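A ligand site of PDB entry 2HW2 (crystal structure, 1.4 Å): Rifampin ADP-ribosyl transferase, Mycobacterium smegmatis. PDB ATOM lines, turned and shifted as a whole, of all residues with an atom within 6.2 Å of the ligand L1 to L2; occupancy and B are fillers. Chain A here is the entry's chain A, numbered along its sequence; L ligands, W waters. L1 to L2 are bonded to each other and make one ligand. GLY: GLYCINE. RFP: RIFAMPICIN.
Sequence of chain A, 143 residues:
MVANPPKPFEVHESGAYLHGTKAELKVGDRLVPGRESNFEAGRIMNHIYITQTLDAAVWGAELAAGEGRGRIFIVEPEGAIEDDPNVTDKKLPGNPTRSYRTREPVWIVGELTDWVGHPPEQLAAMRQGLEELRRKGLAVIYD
The side-chain amide nitrogen of Asn 38 lies within hydrogen-bond range of an oxygen (OXT) of GLY L2. O of GLY L2 lies within hydrogen-bond range of N of Asn 38. OD2 of Asp 84 is in salt-bridge range of N of GLY L1, 2.7 Å away. The backbone carbonyl oxygen (O) of Asn 86 is in hydrogen-bond range of an oxygen (O1) of RFP L3, at 3.2 Å.
CA of Ser 37 touches O of GLY L2, 3.7 Å away. CD1 of Phe 39 touches C of GLY L2, 3.8 Å away. CE of Met 45 touches O of GLY L2 (3.8 Å). Tyr 49 touches the ligand L1 to L2. Asn 86 touches the ligand L1 to L2. Hydrophobic or aromatic side chains within 4 Å of the ligand L1 to L2: Phe 39, Met 45 and Tyr 49. Of the 13 residues printed, 7 come within 4 Å of the ligand L1 to L2.
Water W5 lies within hydrogen-bond range of OG of Ser 37, O of GLY L2 and SD of Met 45. Water W3 lies within hydrogen-bond range of O of Glu 36 (2.9 Å), O of GLY L2 (3.0 Å) and ND2 of Asn 38 (3.4 Å). Water W1 lies within hydrogen-bond range of O of GLY L1 (3.0 Å) and O of Tyr 142 (3.4 Å).
An oxygen (O8) of RFP L3 is in hydrogen-bond range of a nitrogen (N) of GLY L1 (2.7 Å).
The backbone NH of Asp 84 is in hydrogen-bond range of the backbone carbonyl oxygen of Ser 99 (3.0 Å). OG of Ser 37 sits at hydrogen-bond distance from N of Phe 39. The side-chain carboxylate of Asp 84 lies within hydrogen-bond range of the backbone NH of Asn 86 (2.9 Å). O of Tyr 142 lies within hydrogen-bond range of ND2 of Asn 86 (2.9 Å). The side-chain hydroxyl (OH) of Tyr 49 is in hydrogen-bond range of the backbone carbonyl oxygen (O) of Tyr 142 (3.3 Å).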
ATOM      1  N   GLY A  20       4.051 -32.535   0.780  1.00  0.00           N
ATOM      2  CA  GLY A  20       3.892 -33.440   1.901  1.00  0.00           C
ATOM      3  C   GLY A  20       3.965 -32.653   3.206  1.00  0.00           C
ATOM      4  O   GLY A  20       4.748 -31.715   3.364  1.00  0.00           O
ATOM      5  N   GLU A  36       5.649 -22.119  10.309  1.00  0.00           N
ATOM      6  CA  GLU A  36       6.936 -22.462  10.935  1.00  0.00           C
ATOM      7  C   GLU A  36       7.681 -23.569  10.157  1.00  0.00           C
ATOM      8  O   GLU A  36       7.084 -24.478   9.571  1.00  0.00           O
ATOM      9  CB  GLU A  36       6.660 -22.932  12.389  1.00  0.00           C
ATOM     10  CG  GLU A  36       7.955 -23.207  13.161  1.00  0.00           C
ATOM     11  CD  GLU A  36       7.711 -23.522  14.613  1.00  0.00           C
ATOM     12  OE1 GLU A  36       6.517 -23.641  14.989  1.00  0.00           O
ATOM     13  OE2 GLU A  36       8.643 -23.695  15.391  1.00  0.00           O
ATOM     14  N   SER A  37       9.003 -23.439  10.090  1.00  0.00           N
ATOM     15  CA  SER A  37       9.851 -24.451   9.559  1.00  0.00           C
ATOM     16  C   SER A  37       9.621 -25.804  10.131  1.00  0.00           C
ATOM     17  O   SER A  37       9.474 -25.934  11.339  1.00  0.00           O
ATOM     18  CB  SER A  37      11.314 -24.018   9.836  1.00  0.00           C
ATOM     19  OG  SER A  37      12.216 -24.997   9.315  1.00  0.00           O
ATOM     20  N   ASN A  38       9.718 -26.835   9.307  1.00  0.00           N
ATOM     21  CA  ASN A  38       9.770 -28.233   9.807  1.00  0.00           C
ATOM     22  C   ASN A  38      11.121 -28.683  10.294  1.00  0.00           C
ATOM     23  O   ASN A  38      11.246 -29.812  10.861  1.00  0.00           O
ATOM     24  CB  ASN A  38       9.253 -29.166   8.689  1.00  0.00           C
ATOM     25  CG  ASN A  38       7.803 -29.005   8.494  1.00  0.00           C
ATOM     26  OD1 ASN A  38       7.027 -29.220   9.436  1.00  0.00           O
ATOM     27  ND2 ASN A  38       7.410 -28.471   7.344  1.00  0.00           N
ATOM     28  N   PHE A  39      12.160 -27.834  10.065  1.00  0.00           N
ATOM     29  CA  PHE A  39      13.542 -28.302  10.307  1.00  0.00           C
ATOM     30  C   PHE A  39      14.328 -27.402  11.250  1.00  0.00           C
ATOM     31  O   PHE A  39      15.444 -27.796  11.665  1.00  0.00           O
ATOM     32  CB  PHE A  39      14.293 -28.420   8.986  1.00  0.00           C
ATOM     33  CG  PHE A  39      13.706 -29.472   8.106  1.00  0.00           C
ATOM     34  CD1 PHE A  39      12.805 -29.146   7.132  1.00  0.00           C
ATOM     35  CD2 PHE A  39      14.034 -30.823   8.353  1.00  0.00           C
ATOM     36  CE1 PHE A  39      12.215 -30.145   6.366  1.00  0.00           C
ATOM     37  CE2 PHE A  39      13.431 -31.834   7.612  1.00  0.00           C
ATOM     38  CZ  PHE A  39      12.532 -31.493   6.621  1.00  0.00           C
ATOM     39  N   MET A  45       8.830 -19.175   7.742  1.00  0.00           N
ATOM     40  CA  MET A  45       9.186 -19.459   6.341  1.00  0.00           C
ATOM     41  C   MET A  45       8.691 -18.445   5.341  1.00  0.00           C
ATOM     42  O   MET A  45       7.559 -17.941   5.471  1.00  0.00           O
ATOM     43  CB  MET A  45       8.633 -20.813   5.915  1.00  0.00           C
ATOM     44  CG  MET A  45       9.136 -21.951   6.842  1.00  0.00           C
ATOM     45  SD  MET A  45      10.941 -22.184   6.810  1.00  0.00           S
ATOM     46  CE  MET A  45      11.130 -22.916   5.187  1.00  0.00           C
ATOM     47  N   TYR A  49       7.013 -25.220  -0.027  1.00  0.00           N
ATOM     48  CA  TYR A  49       7.919 -26.169  -0.698  1.00  0.00           C
ATOM     49  C   TYR A  49       7.054 -27.246  -1.336  1.00  0.00           C
ATOM     50  O   TYR A  49       6.147 -27.840  -0.689  1.00  0.00           O
ATOM     51  CB  TYR A  49       8.908 -26.753   0.334  1.00  0.00           C
ATOM     52  CG  TYR A  49       9.891 -25.682   0.693  1.00  0.00           C
ATOM     53  CD1 TYR A  49       9.576 -24.688   1.633  1.00  0.00           C
ATOM     54  CD2 TYR A  49      11.150 -25.659   0.081  1.00  0.00           C
ATOM     55  CE1 TYR A  49      10.492 -23.594   1.858  1.00  0.00           C
ATOM     56  CE2 TYR A  49      12.070 -24.626   0.367  1.00  0.00           C
ATOM     57  CZ  TYR A  49      11.742 -23.609   1.225  1.00  0.00           C
ATOM     58  OH  TYR A  49      12.632 -22.559   1.446  1.00  0.00           O
ATOM     59  N   ASP A  84      14.398 -25.467  -5.335  1.00  0.00           N
ATOM     60  CA  ASP A  84      14.705 -25.412  -3.919  1.00  0.00           C
ATOM     61  C   ASP A  84      16.212 -25.547  -3.721  1.00  0.00           C
ATOM     62  O   ASP A  84      16.785 -26.625  -3.973  1.00  0.00           O
ATOM     63  CB  ASP A  84      14.008 -26.644  -3.320  1.00  0.00           C
ATOM     64  CG  ASP A  84      14.226 -26.829  -1.816  1.00  0.00           C
ATOM     65  OD1 ASP A  84      15.070 -26.080  -1.220  1.00  0.00           O
ATOM     66  OD2 ASP A  84      13.527 -27.704  -1.236  1.00  0.00           O
ATOM     67  N   ASN A  86      17.974 -25.994  -1.191  1.00  0.00           N
ATOM     68  CA  ASN A  86      18.486 -27.003  -0.208  1.00  0.00           C
ATOM     69  C   ASN A  86      18.860 -28.325  -0.866  1.00  0.00           C
ATOM     70  O   ASN A  86      19.678 -29.082  -0.335  1.00  0.00           O
ATOM     71  CB  ASN A  86      17.458 -27.280   0.900  1.00  0.00           C
ATOM     72  CG  ASN A  86      17.202 -26.042   1.705  1.00  0.00           C
ATOM     73  OD1 ASN A  86      18.032 -25.643   2.487  1.00  0.00           O
ATOM     74  ND2 ASN A  86      16.104 -25.336   1.399  1.00  0.00           N
ATOM     75  N   VAL A  87      18.300 -28.577  -2.063  1.00  0.00           N
ATOM     76  CA  VAL A  87      18.547 -29.875  -2.698  1.00  0.00           C
ATOM     77  C   VAL A  87      18.958 -29.708  -4.185  1.00  0.00           C
ATOM     78  O   VAL A  87      18.854 -30.659  -4.952  1.00  0.00           O
ATOM     79  CB  VAL A  87      17.361 -30.868  -2.523  1.00  0.00           C
ATOM     80  CG1 VAL A  87      17.260 -31.226  -0.998  1.00  0.00           C
ATOM     81  CG2 VAL A  87      16.066 -30.278  -3.098  1.00  0.00           C
ATOM     82  N   SER A  99      12.462 -30.597  -6.722  1.00  0.00           N
ATOM     83  CA  SER A  99      11.945 -29.896  -5.586  1.00  0.00           C
ATOM     84  C   SER A  99      11.978 -28.412  -5.836  1.00  0.00           C
ATOM     85  O   SER A  99      12.984 -27.889  -6.293  1.00  0.00           O
ATOM     86  CB  SER A  99      12.776 -30.192  -4.315  1.00  0.00           C
ATOM     87  OG  SER A  99      12.610 -31.549  -3.943  1.00  0.00           O
ATOM     88  N   ILE A 141      19.576 -24.110   6.892  1.00  0.00           N
ATOM     89  CA  ILE A 141      18.286 -24.053   6.179  1.00  0.00           C
ATOM     90  C   ILE A 141      18.278 -22.830   5.258  1.00  0.00           C
ATOM     91  O   ILE A 141      18.392 -21.671   5.721  1.00  0.00           O
ATOM     92  CB  ILE A 141      17.107 -23.976   7.169  1.00  0.00           C
ATOM     93  CG1 ILE A 141      16.816 -25.384   7.822  1.00  0.00           C
ATOM     94  CG2 ILE A 141      15.784 -23.613   6.391  1.00  0.00           C
ATOM     95  CD1 ILE A 141      17.693 -25.861   8.861  1.00  0.00           C
ATOM     96  N   TYR A 142      18.178 -23.067   3.946  1.00  0.00           N
ATOM     97  CA  TYR A 142      18.019 -21.985   3.014  1.00  0.00           C
ATOM     98  C   TYR A 142      16.550 -21.708   2.815  1.00  0.00           C
ATOM     99  O   TYR A 142      15.777 -22.608   2.433  1.00  0.00           O
ATOM    100  CB  TYR A 142      18.739 -22.312   1.698  1.00  0.00           C
ATOM    101  CG  TYR A 142      20.236 -22.273   1.889  1.00  0.00           C
ATOM    102  CD1 TYR A 142      20.981 -23.434   1.965  1.00  0.00           C
ATOM    103  CD2 TYR A 142      20.902 -21.057   2.003  1.00  0.00           C
ATOM    104  CE1 TYR A 142      22.364 -23.393   2.145  1.00  0.00           C
ATOM    105  CE2 TYR A 142      22.310 -21.009   2.151  1.00  0.00           C
ATOM    106  CZ  TYR A 142      23.001 -22.193   2.236  1.00  0.00           C
ATOM    107  OH  TYR A 142      24.376 -22.132   2.422  1.00  0.00           O
HETATM  108  N   GLY L   1      13.357 -29.414   0.785  1.00  0.00           N
HETATM  109  CA  GLY L   1      12.022 -29.238   1.449  1.00  0.00           C
HETATM  110  C   GLY L   1      12.116 -28.135   2.465  1.00  0.00           C
HETATM  111  O   GLY L   1      13.087 -27.343   2.398  1.00  0.00           O
HETATM  112  N   GLY L   2      11.133 -28.000   3.338  1.00  0.00           N
HETATM  113  CA  GLY L   2      11.174 -26.884   4.335  1.00  0.00           C
HETATM  114  C   GLY L   2      10.111 -27.050   5.392  1.00  0.00           C
HETATM  115  O   GLY L   2      10.175 -26.356   6.432  1.00  0.00           O
HETATM  116  OXT GLY L   2       9.166 -27.867   5.237  1.00  0.00           O
HETATM  117  C1  RFP L   3      21.083 -32.907   0.710  1.00  0.00           C
HETATM  118  C2  RFP L   3      21.169 -33.177   2.077  1.00  0.00           C
HETATM  119  C3  RFP L   3      20.725 -34.403   2.562  1.00  0.00           C
HETATM  120  C4  RFP L   3      20.228 -35.382   1.689  1.00  0.00           C
HETATM  121  C5  RFP L   3      19.589 -36.005  -0.661  1.00  0.00           C
HETATM  122  C6  RFP L   3      19.436 -35.632  -1.966  1.00  0.00           C
HETATM  123  C7  RFP L   3      19.899 -34.420  -2.444  1.00  0.00           C
HETATM  124  C8  RFP L   3      20.457 -33.553  -1.557  1.00  0.00           C
HETATM  125  C9  RFP L   3      20.549 -33.857  -0.178  1.00  0.00           C
HETATM  126  C10 RFP L   3      20.115 -35.111   0.296  1.00  0.00           C
HETATM  127  C11 RFP L   3      18.945 -37.363  -0.557  1.00  0.00           C
HETATM  128  C12 RFP L   3      18.263 -37.661  -1.870  1.00  0.00           C
HETATM  129  C13 RFP L   3      18.544 -39.038  -2.444  1.00  0.00           C
HETATM  130  C14 RFP L   3      19.804 -34.097  -3.913  1.00  0.00           C
HETATM  131  C15 RFP L   3      22.607 -32.142   3.773  1.00  0.00           C
HETATM  132  C16 RFP L   3      22.885 -30.922   4.562  1.00  0.00           C
HETATM  133  C17 RFP L   3      21.982 -30.103   5.118  1.00  0.00           C
HETATM  134  C18 RFP L   3      20.498 -30.290   5.132  1.00  0.00           C
HETATM  135  C19 RFP L   3      19.758 -29.287   5.632  1.00  0.00           C
HETATM  136  C20 RFP L   3      18.212 -29.183   5.753  1.00  0.00           C
HETATM  137  C21 RFP L   3      17.529 -30.069   4.681  1.00  0.00           C
HETATM  138  C22 RFP L   3      15.989 -30.069   4.769  1.00  0.00           C
HETATM  139  C23 RFP L   3      15.340 -30.897   3.654  1.00  0.00           C
HETATM  140  C24 RFP L   3      15.910 -32.352   3.526  1.00  0.00           C
HETATM  141  C25 RFP L   3      15.148 -33.132   2.393  1.00  0.00           C
HETATM  142  C26 RFP L   3      15.690 -34.523   2.011  1.00  0.00           C
HETATM  143  C27 RFP L   3      14.928 -35.068   0.764  1.00  0.00           C
HETATM  144  C28 RFP L   3      15.432 -36.453   0.248  1.00  0.00           C
HETATM  145  C29 RFP L   3      16.186 -36.453  -0.892  1.00  0.00           C
HETATM  146  C30 RFP L   3      24.338 -30.561   4.730  1.00  0.00           C
HETATM  147  C31 RFP L   3      17.830 -29.652   7.167  1.00  0.00           C
HETATM  148  C32 RFP L   3      15.415 -28.620   4.740  1.00  0.00           C
HETATM  149  C33 RFP L   3      15.754 -33.060   4.893  1.00  0.00           C
HETATM  150  C34 RFP L   3      17.166 -34.326   1.671  1.00  0.00           C
HETATM  151  C35 RFP L   3      12.688 -32.746   2.278  1.00  0.00           C
HETATM  152  C36 RFP L   3      11.361 -33.087   2.916  1.00  0.00           C
HETATM  153  C37 RFP L   3      13.968 -34.055  -1.169  1.00  0.00           C
HETATM  154  C38 RFP L   3      21.202 -38.934   5.041  1.00  0.00           C
HETATM  155  C39 RFP L   3      22.653 -37.742   6.759  1.00  0.00           C
HETATM  156  C40 RFP L   3      22.866 -36.273   6.428  1.00  0.00           C
HETATM  157  C41 RFP L   3      20.373 -35.942   6.615  1.00  0.00           C
HETATM  158  C42 RFP L   3      20.166 -37.447   6.829  1.00  0.00           C
HETATM  159  C43 RFP L   3      20.840 -34.602   4.014  1.00  0.00           C
HETATM  160  N1  RFP L   3      21.619 -32.143   2.880  1.00  0.00           N
HETATM  161  N2  RFP L   3      21.482 -35.643   4.412  1.00  0.00           N
HETATM  162  N3  RFP L   3      21.595 -35.914   5.804  1.00  0.00           N
HETATM  163  N4  RFP L   3      21.340 -38.048   6.213  1.00  0.00           N
HETATM  164  O1  RFP L   3      21.509 -31.644   0.336  1.00  0.00           O
HETATM  165  O2  RFP L   3      20.913 -32.374  -2.029  1.00  0.00           O
HETATM  166  O3  RFP L   3      18.866 -36.610  -2.753  1.00  0.00           O
HETATM  167  O4  RFP L   3      18.808 -38.052   0.466  1.00  0.00           O
HETATM  168  O5  RFP L   3      16.796 -37.651  -1.539  1.00  0.00           O
HETATM  169  O6  RFP L   3      15.048 -34.057  -0.256  1.00  0.00           O
HETATM  170  O7  RFP L   3      13.791 -33.388   2.882  1.00  0.00           O
HETATM  171  O8  RFP L   3      12.901 -32.043   1.281  1.00  0.00           O
HETATM  172  O9  RFP L   3      15.506 -30.204   2.375  1.00  0.00           O
HETATM  173  O10 RFP L   3      17.892 -29.643   3.363  1.00  0.00           O
HETATM  174  O11 RFP L   3      23.275 -33.129   3.834  1.00  0.00           O
HETATM  175  O12 RFP L   3      19.846 -36.594   2.180  1.00  0.00           O
HETATM  176  O   HOH W   1      13.759 -24.900   4.013  1.00  0.00           O
HETATM  177  O   HOH W   2       9.561 -30.426   3.329  1.00  0.00           O
HETATM  178  O   HOH W   3       7.515 -25.079   6.723  1.00  0.00           O
HETATM  179  O   HOH W   4       7.041 -28.127   3.476  1.00  0.00           O
HETATM  180  O   HOH W   5      12.696 -25.504   6.778  1.00  0.00           O
